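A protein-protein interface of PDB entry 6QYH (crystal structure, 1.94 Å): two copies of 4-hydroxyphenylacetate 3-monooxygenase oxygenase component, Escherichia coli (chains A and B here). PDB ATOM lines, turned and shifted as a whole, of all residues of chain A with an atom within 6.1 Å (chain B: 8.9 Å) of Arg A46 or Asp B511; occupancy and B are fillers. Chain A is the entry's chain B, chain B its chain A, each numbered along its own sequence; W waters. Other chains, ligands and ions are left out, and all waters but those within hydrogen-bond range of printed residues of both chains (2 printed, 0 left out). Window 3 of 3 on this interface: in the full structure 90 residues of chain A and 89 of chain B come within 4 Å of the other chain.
The backbone NH (N) of His B507 is in hydrogen-bond range of the side-chain amide oxygen (OD1) of Asn A47 (2.8 Å).
NH2 of Arg A46 is in hydrogen-bond range of O of Asn B508 (3.3 Å).
The side-chain carboxylate of Asp B511 lies within salt-bridge range of the guanidinium group of Arg A46 (2.8 Å).
The backbone carbonyl oxygen (O) of His B507 lies within hydrogen-bond range of the indole nitrogen (NE1) of Trp B501, at 3.1 Å.
The backbone NH of Trp B501 is in hydrogen-bond range of the side-chain amide oxygen of Asn B508, at 3.0 Å.
The side-chain carboxylate (OE2) of Glu A242 is in hydrogen-bond range of the backbone NH (N) of Arg A46, 3.3 Å away.
The backbone carbonyl oxygen (O) of Asn A47 lies within hydrogen-bond range of the side-chain hydroxyl (OG) of Ser A51.
The backbone NH (N) of Asn A47 lies within hydrogen-bond range of the side-chain carboxylate (OE2) of Glu A242.
Among the printed residues, pairs that only touch across the chains: Pro A43 with Ile B512, Arg A46 with His B507, Arg A46 with Ile B512, Asn A47 with Leu B506 and Ala A50 with His B505.
Printed residues of chain B within 4 Å of Pro A43: Ile B512.
Arg A46 touches four residues of chain B.
Of the printed residues of chain A, Leu B506 touches Asn A47 (3.8 Å).
Printed residues of chain A within 4 Å of Asp B511: Arg A46 (2.8 Å).
The nearest printed residue of chain A that does not touch His B507 is Thr A40 (4.3 Å).
Hydrophobic or aromatic side chains of chain A within 4 Å of the printed part of chain B: Pro A43 and Ala A50.
Hydrophobic or aromatic side chains of chain B that line the printed part of chain A: His B505, Leu B506, His B507 and Ile B512.
Among the printed residues, 8 pairs touch across the chains.
Among the printed residues, Asp or Glu carboxylates within 4 Å of a Lys or Arg side-chain nitrogen of the other chain: Arg A46 with Asp B511 (2.8 Å).
No position is printed for both chains.
Water W1 lies within hydrogen-bond range of a ring nitrogen (NE2) of His B505 and the side-chain hydroxyl (OG) of Ser A51.
Water W2 lies within hydrogen-bond range of O of His B507 (2.9 Å), NH2 of Arg A46 (3.0 Å) and O of Asn B508 (3.4 Å).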
ATOM      1  N   LEU A  20     -28.919  -2.501 -12.436  1.00  0.00           N
ATOM      2  CA  LEU A  20     -28.613  -3.144 -11.151  1.00  0.00           C
ATOM      3  C   LEU A  20     -28.537  -4.659 -11.278  1.00  0.00           C
ATOM      4  O   LEU A  20     -27.599  -5.248 -10.758  1.00  0.00           O
ATOM      5  CB  LEU A  20     -29.559  -2.704 -10.012  1.00  0.00           C
ATOM      6  CG  LEU A  20     -29.467  -1.214  -9.613  1.00  0.00           C
ATOM      7  CD1 LEU A  20     -30.663  -0.790  -8.775  1.00  0.00           C
ATOM      8  CD2 LEU A  20     -28.138  -0.875  -8.908  1.00  0.00           C
ATOM      9  N   VAL A  39     -22.478  -6.460  -5.304  1.00  0.00           N
ATOM     10  CA  VAL A  39     -22.218  -5.012  -5.217  1.00  0.00           C
ATOM     11  C   VAL A  39     -23.470  -4.177  -4.967  1.00  0.00           C
ATOM     12  O   VAL A  39     -23.385  -3.125  -4.323  1.00  0.00           O
ATOM     13  CB  VAL A  39     -21.407  -4.390  -6.391  1.00  0.00           C
ATOM     14  CG1 VAL A  39     -19.961  -4.809  -6.341  1.00  0.00           C
ATOM     15  CG2 VAL A  39     -22.033  -4.666  -7.762  1.00  0.00           C
ATOM     16  N   THR A  40     -24.628  -4.641  -5.456  1.00  0.00           N
ATOM     17  CA  THR A  40     -25.869  -3.862  -5.340  1.00  0.00           C
ATOM     18  C   THR A  40     -26.457  -3.856  -3.927  1.00  0.00           C
ATOM     19  O   THR A  40     -27.309  -3.019  -3.640  1.00  0.00           O
ATOM     20  CB  THR A  40     -26.893  -4.312  -6.382  1.00  0.00           C
ATOM     21  OG1 THR A  40     -27.427  -5.565  -5.968  1.00  0.00           O
ATOM     22  CG2 THR A  40     -26.304  -4.406  -7.786  1.00  0.00           C
ATOM     23  N   THR A  41     -26.023  -4.778  -3.063  1.00  0.00           N
ATOM     24  CA  THR A  41     -26.509  -4.894  -1.675  1.00  0.00           C
ATOM     25  C   THR A  41     -25.415  -4.637  -0.638  1.00  0.00           C
ATOM     26  O   THR A  41     -25.729  -4.426   0.535  1.00  0.00           O
ATOM     27  CB  THR A  41     -27.161  -6.279  -1.412  1.00  0.00           C
ATOM     28  OG1 THR A  41     -26.145  -7.281  -1.456  1.00  0.00           O
ATOM     29  CG2 THR A  41     -28.319  -6.596  -2.386  1.00  0.00           C
ATOM     30  N   HIS A  42     -24.132  -4.690  -1.049  1.00  0.00           N
ATOM     31  CA  HIS A  42     -23.007  -4.500  -0.142  1.00  0.00           C
ATOM     32  C   HIS A  42     -23.006  -3.060   0.456  1.00  0.00           C
ATOM     33  O   HIS A  42     -23.188  -2.100  -0.288  1.00  0.00           O
ATOM     34  CB  HIS A  42     -21.673  -4.796  -0.865  1.00  0.00           C
ATOM     35  CG  HIS A  42     -20.499  -4.905   0.053  1.00  0.00           C
ATOM     36  ND1 HIS A  42     -19.899  -3.778   0.608  1.00  0.00           N
ATOM     37  CD2 HIS A  42     -19.860  -6.011   0.509  1.00  0.00           C
ATOM     38  CE1 HIS A  42     -18.916  -4.234   1.377  1.00  0.00           C
ATOM     39  NE2 HIS A  42     -18.839  -5.567   1.335  1.00  0.00           N
ATOM     40  N   PRO A  43     -22.803  -2.916   1.789  1.00  0.00           N
ATOM     41  CA  PRO A  43     -22.840  -1.568   2.408  1.00  0.00           C
ATOM     42  C   PRO A  43     -21.806  -0.545   1.909  1.00  0.00           C
ATOM     43  O   PRO A  43     -21.985   0.642   2.186  1.00  0.00           O
ATOM     44  CB  PRO A  43     -22.664  -1.847   3.912  1.00  0.00           C
ATOM     45  CG  PRO A  43     -22.137  -3.253   4.007  1.00  0.00           C
ATOM     46  CD  PRO A  43     -22.616  -3.983   2.803  1.00  0.00           C
ATOM     47  N   ALA A  44     -20.748  -0.973   1.177  1.00  0.00           N
ATOM     48  CA  ALA A  44     -19.741  -0.053   0.612  1.00  0.00           C
ATOM     49  C   ALA A  44     -20.111   0.473  -0.792  1.00  0.00           C
ATOM     50  O   ALA A  44     -19.497   1.430  -1.251  1.00  0.00           O
ATOM     51  CB  ALA A  44     -18.388  -0.745   0.531  1.00  0.00           C
ATOM     52  N   PHE A  45     -21.058  -0.172  -1.490  1.00  0.00           N
ATOM     53  CA  PHE A  45     -21.362   0.179  -2.887  1.00  0.00           C
ATOM     54  C   PHE A  45     -22.828   0.390  -3.244  1.00  0.00           C
ATOM     55  O   PHE A  45     -23.099   0.894  -4.346  1.00  0.00           O
ATOM     56  CB  PHE A  45     -20.844  -0.970  -3.795  1.00  0.00           C
ATOM     57  CG  PHE A  45     -19.356  -1.240  -3.695  1.00  0.00           C
ATOM     58  CD1 PHE A  45     -18.436  -0.451  -4.391  1.00  0.00           C
ATOM     59  CD2 PHE A  45     -18.874  -2.278  -2.902  1.00  0.00           C
ATOM     60  CE1 PHE A  45     -17.063  -0.689  -4.278  1.00  0.00           C
ATOM     61  CE2 PHE A  45     -17.499  -2.519  -2.799  1.00  0.00           C
ATOM     62  CZ  PHE A  45     -16.606  -1.730  -3.488  1.00  0.00           C
ATOM     63  N   ARG A  46     -23.765  -0.067  -2.387  1.00  0.00           N
ATOM     64  CA  ARG A  46     -25.212  -0.098  -2.706  1.00  0.00           C
ATOM     65  C   ARG A  46     -25.826   1.270  -3.087  1.00  0.00           C
ATOM     66  O   ARG A  46     -26.612   1.324  -4.012  1.00  0.00           O
ATOM     67  CB  ARG A  46     -26.023  -0.776  -1.586  1.00  0.00           C
ATOM     68  CG  ARG A  46     -25.951  -0.078  -0.237  1.00  0.00           C
ATOM     69  CD  ARG A  46     -26.567  -0.913   0.858  1.00  0.00           C
ATOM     70  NE  ARG A  46     -26.634  -0.154   2.105  1.00  0.00           N
ATOM     71  CZ  ARG A  46     -27.303  -0.548   3.183  1.00  0.00           C
ATOM     72  NH1 ARG A  46     -27.952  -1.705   3.184  1.00  0.00           N
ATOM     73  NH2 ARG A  46     -27.331   0.212   4.266  1.00  0.00           N
ATOM     74  N   ASN A  47     -25.475   2.354  -2.384  1.00  0.00           N
ATOM     75  CA  ASN A  47     -26.023   3.685  -2.690  1.00  0.00           C
ATOM     76  C   ASN A  47     -25.374   4.308  -3.914  1.00  0.00           C
ATOM     77  O   ASN A  47     -26.085   4.939  -4.690  1.00  0.00           O
ATOM     78  CB  ASN A  47     -25.992   4.616  -1.478  1.00  0.00           C
ATOM     79  CG  ASN A  47     -27.040   4.280  -0.450  1.00  0.00           C
ATOM     80  OD1 ASN A  47     -28.038   3.623  -0.740  1.00  0.00           O
ATOM     81  ND2 ASN A  47     -26.848   4.723   0.771  1.00  0.00           N
ATOM     82  N   ALA A  48     -24.043   4.108  -4.113  1.00  0.00           N
ATOM     83  CA  ALA A  48     -23.343   4.564  -5.326  1.00  0.00           C
ATOM     84  C   ALA A  48     -23.963   3.822  -6.533  1.00  0.00           C
ATOM     85  O   ALA A  48     -24.216   4.442  -7.576  1.00  0.00           O
ATOM     86  CB  ALA A  48     -21.859   4.261  -5.225  1.00  0.00           C
ATOM     87  N   ALA A  49     -24.258   2.508  -6.367  1.00  0.00           N
ATOM     88  CA  ALA A  49     -24.917   1.702  -7.418  1.00  0.00           C
ATOM     89  C   ALA A  49     -26.320   2.253  -7.696  1.00  0.00           C
ATOM     90  O   ALA A  49     -26.681   2.454  -8.862  1.00  0.00           O
ATOM     91  CB  ALA A  49     -24.998   0.234  -7.015  1.00  0.00           C
ATOM     92  N   ALA A  50     -27.085   2.564  -6.619  1.00  0.00           N
ATOM     93  CA  ALA A  50     -28.426   3.164  -6.732  1.00  0.00           C
ATOM     94  C   ALA A  50     -28.367   4.559  -7.410  1.00  0.00           C
ATOM     95  O   ALA A  50     -29.252   4.879  -8.196  1.00  0.00           O
ATOM     96  CB  ALA A  50     -29.083   3.255  -5.359  1.00  0.00           C
ATOM     97  N   SER A  51     -27.300   5.371  -7.134  1.00  0.00           N
ATOM     98  CA  SER A  51     -27.116   6.688  -7.756  1.00  0.00           C
ATOM     99  C   SER A  51     -26.895   6.580  -9.268  1.00  0.00           C
ATOM    100  O   SER A  51     -27.508   7.341 -10.022  1.00  0.00           O
ATOM    101  CB  SER A  51     -25.970   7.455  -7.095  1.00  0.00           C
ATOM    102  OG  SER A  51     -26.346   7.799  -5.775  1.00  0.00           O
ATOM    103  N   GLU A 242     -18.726   5.590   1.721  1.00  0.00           N
ATOM    104  CA  GLU A 242     -20.138   5.240   1.813  1.00  0.00           C
ATOM    105  C   GLU A 242     -20.360   4.339   3.036  1.00  0.00           C
ATOM    106  O   GLU A 242     -21.269   4.589   3.828  1.00  0.00           O
ATOM    107  CB  GLU A 242     -20.615   4.525   0.535  1.00  0.00           C
ATOM    108  CG  GLU A 242     -22.061   4.021   0.678  1.00  0.00           C
ATOM    109  CD  GLU A 242     -22.708   3.388  -0.535  1.00  0.00           C
ATOM    110  OE1 GLU A 242     -22.309   3.716  -1.676  1.00  0.00           O
ATOM    111  OE2 GLU A 242     -23.639   2.577  -0.340  1.00  0.00           O
ATOM    112  N   TRP B 501     -33.108   9.337   4.565  1.00  0.00           N
ATOM    113  CA  TRP B 501     -33.453   9.732   3.201  1.00  0.00           C
ATOM    114  C   TRP B 501     -34.947  10.061   3.094  1.00  0.00           C
ATOM    115  O   TRP B 501     -35.756   9.477   3.809  1.00  0.00           O
ATOM    116  CB  TRP B 501     -33.105   8.595   2.204  1.00  0.00           C
ATOM    117  CG  TRP B 501     -31.644   8.240   2.151  1.00  0.00           C
ATOM    118  CD1 TRP B 501     -31.083   7.053   2.519  1.00  0.00           C
ATOM    119  CD2 TRP B 501     -30.556   9.094   1.750  1.00  0.00           C
ATOM    120  NE1 TRP B 501     -29.717   7.104   2.357  1.00  0.00           N
ATOM    121  CE2 TRP B 501     -29.366   8.339   1.878  1.00  0.00           C
ATOM    122  CE3 TRP B 501     -30.469  10.430   1.296  1.00  0.00           C
ATOM    123  CZ2 TRP B 501     -28.098   8.875   1.592  1.00  0.00           C
ATOM    124  CZ3 TRP B 501     -29.210  10.959   1.010  1.00  0.00           C
ATOM    125  CH2 TRP B 501     -28.045  10.189   1.167  1.00  0.00           C
ATOM    126  N   HIS B 505     -35.111   5.715  -3.594  1.00  0.00           N
ATOM    127  CA  HIS B 505     -34.102   4.894  -4.264  1.00  0.00           C
ATOM    128  C   HIS B 505     -32.863   4.581  -3.414  1.00  0.00           C
ATOM    129  O   HIS B 505     -32.108   3.668  -3.770  1.00  0.00           O
ATOM    130  CB  HIS B 505     -33.711   5.517  -5.616  1.00  0.00           C
ATOM    131  CG  HIS B 505     -32.823   6.725  -5.523  1.00  0.00           C
ATOM    132  ND1 HIS B 505     -33.333   7.976  -5.220  1.00  0.00           N
ATOM    133  CD2 HIS B 505     -31.491   6.837  -5.732  1.00  0.00           C
ATOM    134  CE1 HIS B 505     -32.304   8.807  -5.264  1.00  0.00           C
ATOM    135  NE2 HIS B 505     -31.180   8.170  -5.592  1.00  0.00           N
ATOM    136  N   LEU B 506     -32.672   5.285  -2.284  1.00  0.00           N
ATOM    137  CA  LEU B 506     -31.478   5.093  -1.450  1.00  0.00           C
ATOM    138  C   LEU B 506     -31.737   4.265  -0.203  1.00  0.00           C
ATOM    139  O   LEU B 506     -32.844   4.294   0.344  1.00  0.00           O
ATOM    140  CB  LEU B 506     -30.815   6.447  -1.106  1.00  0.00           C
ATOM    141  CG  LEU B 506     -30.348   7.278  -2.320  1.00  0.00           C
ATOM    142  CD1 LEU B 506     -30.122   8.744  -1.937  1.00  0.00           C
ATOM    143  CD2 LEU B 506     -29.088   6.680  -2.961  1.00  0.00           C
ATOM    144  N   HIS B 507     -30.713   3.513   0.226  1.00  0.00           N
ATOM    145  CA  HIS B 507     -30.773   2.644   1.398  1.00  0.00           C
ATOM    146  C   HIS B 507     -30.450   3.419   2.653  1.00  0.00           C
ATOM    147  O   HIS B 507     -29.379   4.026   2.759  1.00  0.00           O
ATOM    148  CB  HIS B 507     -29.788   1.454   1.279  1.00  0.00           C
ATOM    149  CG  HIS B 507     -29.985   0.631   0.051  1.00  0.00           C
ATOM    150  ND1 HIS B 507     -30.663  -0.571   0.096  1.00  0.00           N
ATOM    151  CD2 HIS B 507     -29.599   0.872  -1.227  1.00  0.00           C
ATOM    152  CE1 HIS B 507     -30.669  -1.027  -1.150  1.00  0.00           C
ATOM    153  NE2 HIS B 507     -30.049  -0.187  -1.983  1.00  0.00           N
ATOM    154  N   ASN B 508     -31.356   3.352   3.625  1.00  0.00           N
ATOM    155  CA  ASN B 508     -31.140   3.944   4.947  1.00  0.00           C
ATOM    156  C   ASN B 508     -30.101   3.108   5.701  1.00  0.00           C
ATOM    157  O   ASN B 508     -29.887   1.953   5.348  1.00  0.00           O
ATOM    158  CB  ASN B 508     -32.468   4.069   5.705  1.00  0.00           C
ATOM    159  CG  ASN B 508     -33.233   5.296   5.252  1.00  0.00           C
ATOM    160  OD1 ASN B 508     -32.792   6.431   5.431  1.00  0.00           O
ATOM    161  ND2 ASN B 508     -34.378   5.101   4.630  1.00  0.00           N
ATOM    162  N   ASN B 509     -29.429   3.698   6.686  1.00  0.00           N
ATOM    163  CA  ASN B 509     -28.355   3.025   7.411  1.00  0.00           C
ATOM    164  C   ASN B 509     -28.780   2.227   8.660  1.00  0.00           C
ATOM    165  O   ASN B 509     -27.902   1.770   9.390  1.00  0.00           O
ATOM    166  CB  ASN B 509     -27.279   4.061   7.776  1.00  0.00           C
ATOM    167  CG  ASN B 509     -27.699   5.044   8.839  1.00  0.00           C
ATOM    168  OD1 ASN B 509     -28.873   5.205   9.185  1.00  0.00           O
ATOM    169  ND2 ASN B 509     -26.742   5.709   9.398  1.00  0.00           N
ATOM    170  N   ASP B 510     -30.095   2.051   8.906  1.00  0.00           N
ATOM    171  CA  ASP B 510     -30.612   1.316  10.072  1.00  0.00           C
ATOM    172  C   ASP B 510     -30.044  -0.096  10.204  1.00  0.00           C
ATOM    173  O   ASP B 510     -29.812  -0.561  11.324  1.00  0.00           O
ATOM    174  CB  ASP B 510     -32.153   1.254  10.063  1.00  0.00           C
ATOM    175  CG  ASP B 510     -32.823   2.611   9.973  1.00  0.00           C
ATOM    176  OD1 ASP B 510     -33.560   2.966  10.908  1.00  0.00           O
ATOM    177  OD2 ASP B 510     -32.605   3.318   8.967  1.00  0.00           O
ATOM    178  N   ASP B 511     -29.796  -0.764   9.064  1.00  0.00           N
ATOM    179  CA  ASP B 511     -29.263  -2.128   9.030  1.00  0.00           C
ATOM    180  C   ASP B 511     -27.739  -2.192   9.187  1.00  0.00           C
ATOM    181  O   ASP B 511     -27.199  -3.279   9.403  1.00  0.00           O
ATOM    182  CB  ASP B 511     -29.719  -2.836   7.735  1.00  0.00           C
ATOM    183  CG  ASP B 511     -29.288  -2.146   6.429  1.00  0.00           C
ATOM    184  OD1 ASP B 511     -28.801  -0.994   6.491  1.00  0.00           O
ATOM    185  OD2 ASP B 511     -29.460  -2.755   5.347  1.00  0.00           O
ATOM    186  N   ILE B 512     -27.028  -1.042   9.071  1.00  0.00           N
ATOM    187  CA  ILE B 512     -25.564  -1.057   9.151  1.00  0.00           C
ATOM    188  C   ILE B 512     -24.976  -0.116  10.222  1.00  0.00           C
ATOM    189  O   ILE B 512     -23.795  -0.270  10.552  1.00  0.00           O
ATOM    190  CB  ILE B 512     -24.880  -0.821   7.767  1.00  0.00           C
ATOM    191  CG1 ILE B 512     -25.241   0.576   7.160  1.00  0.00           C
ATOM    192  CG2 ILE B 512     -25.173  -1.989   6.790  1.00  0.00           C
ATOM    193  CD1 ILE B 512     -24.391   1.032   5.916  1.00  0.00           C
ATOM    194  N   ASN B 513     -25.760   0.852  10.743  1.00  0.00           N
ATOM    195  CA  ASN B 513     -25.242   1.780  11.753  1.00  0.00           C
ATOM    196  C   ASN B 513     -24.967   1.022  13.040  1.00  0.00           C
ATOM    197  O   ASN B 513     -25.858   0.373  13.574  1.00  0.00           O
ATOM    198  CB  ASN B 513     -26.124   3.012  11.942  1.00  0.00           C
ATOM    199  CG  ASN B 513     -25.464   4.039  12.815  1.00  0.00           C
ATOM    200  OD1 ASN B 513     -25.459   3.915  14.038  1.00  0.00           O
ATOM    201  ND2 ASN B 513     -24.882   5.064  12.207  1.00  0.00           N
ATOM    202  N   MET B 514     -23.708   1.088  13.524  1.00  0.00           N
ATOM    203  CA  MET B 514     -23.230   0.362  14.704  1.00  0.00           C
ATOM    204  C   MET B 514     -23.151   1.166  16.010  1.00  0.00           C
ATOM    205  O   MET B 514     -22.699   0.607  17.017  1.00  0.00           O
ATOM    206  CB  MET B 514     -21.851  -0.264  14.406  1.00  0.00           C
ATOM    207  CG  MET B 514     -20.737   0.756  14.211  1.00  0.00           C
ATOM    208  SD  MET B 514     -19.349   0.146  13.209  1.00  0.00           S
ATOM    209  CE  MET B 514     -18.540  -0.930  14.386  1.00  0.00           C
ATOM    210  N   LYS B 517     -25.072  -0.291  19.251  1.00  0.00           N
ATOM    211  CA  LYS B 517     -24.347  -1.469  19.735  1.00  0.00           C
ATOM    212  C   LYS B 517     -23.030  -1.080  20.414  1.00  0.00           C
ATOM    213  O   LYS B 517     -22.665  -1.681  21.418  1.00  0.00           O
ATOM    214  CB  LYS B 517     -24.102  -2.469  18.583  1.00  0.00           C
ATOM    215  CG  LYS B 517     -25.367  -3.211  18.152  1.00  0.00           C
ATOM    216  CD  LYS B 517     -25.165  -4.072  16.915  1.00  0.00           C
ATOM    217  CE  LYS B 517     -26.439  -4.804  16.559  1.00  0.00           C
ATOM    218  NZ  LYS B 517     -26.247  -5.742  15.426  1.00  0.00           N
HETATM  219  O   HOH W   1     -28.685   9.353  -5.801  1.00  0.00           O
HETATM  220  O   HOH W   2     -26.997   3.152   4.124  1.00  0.00           O
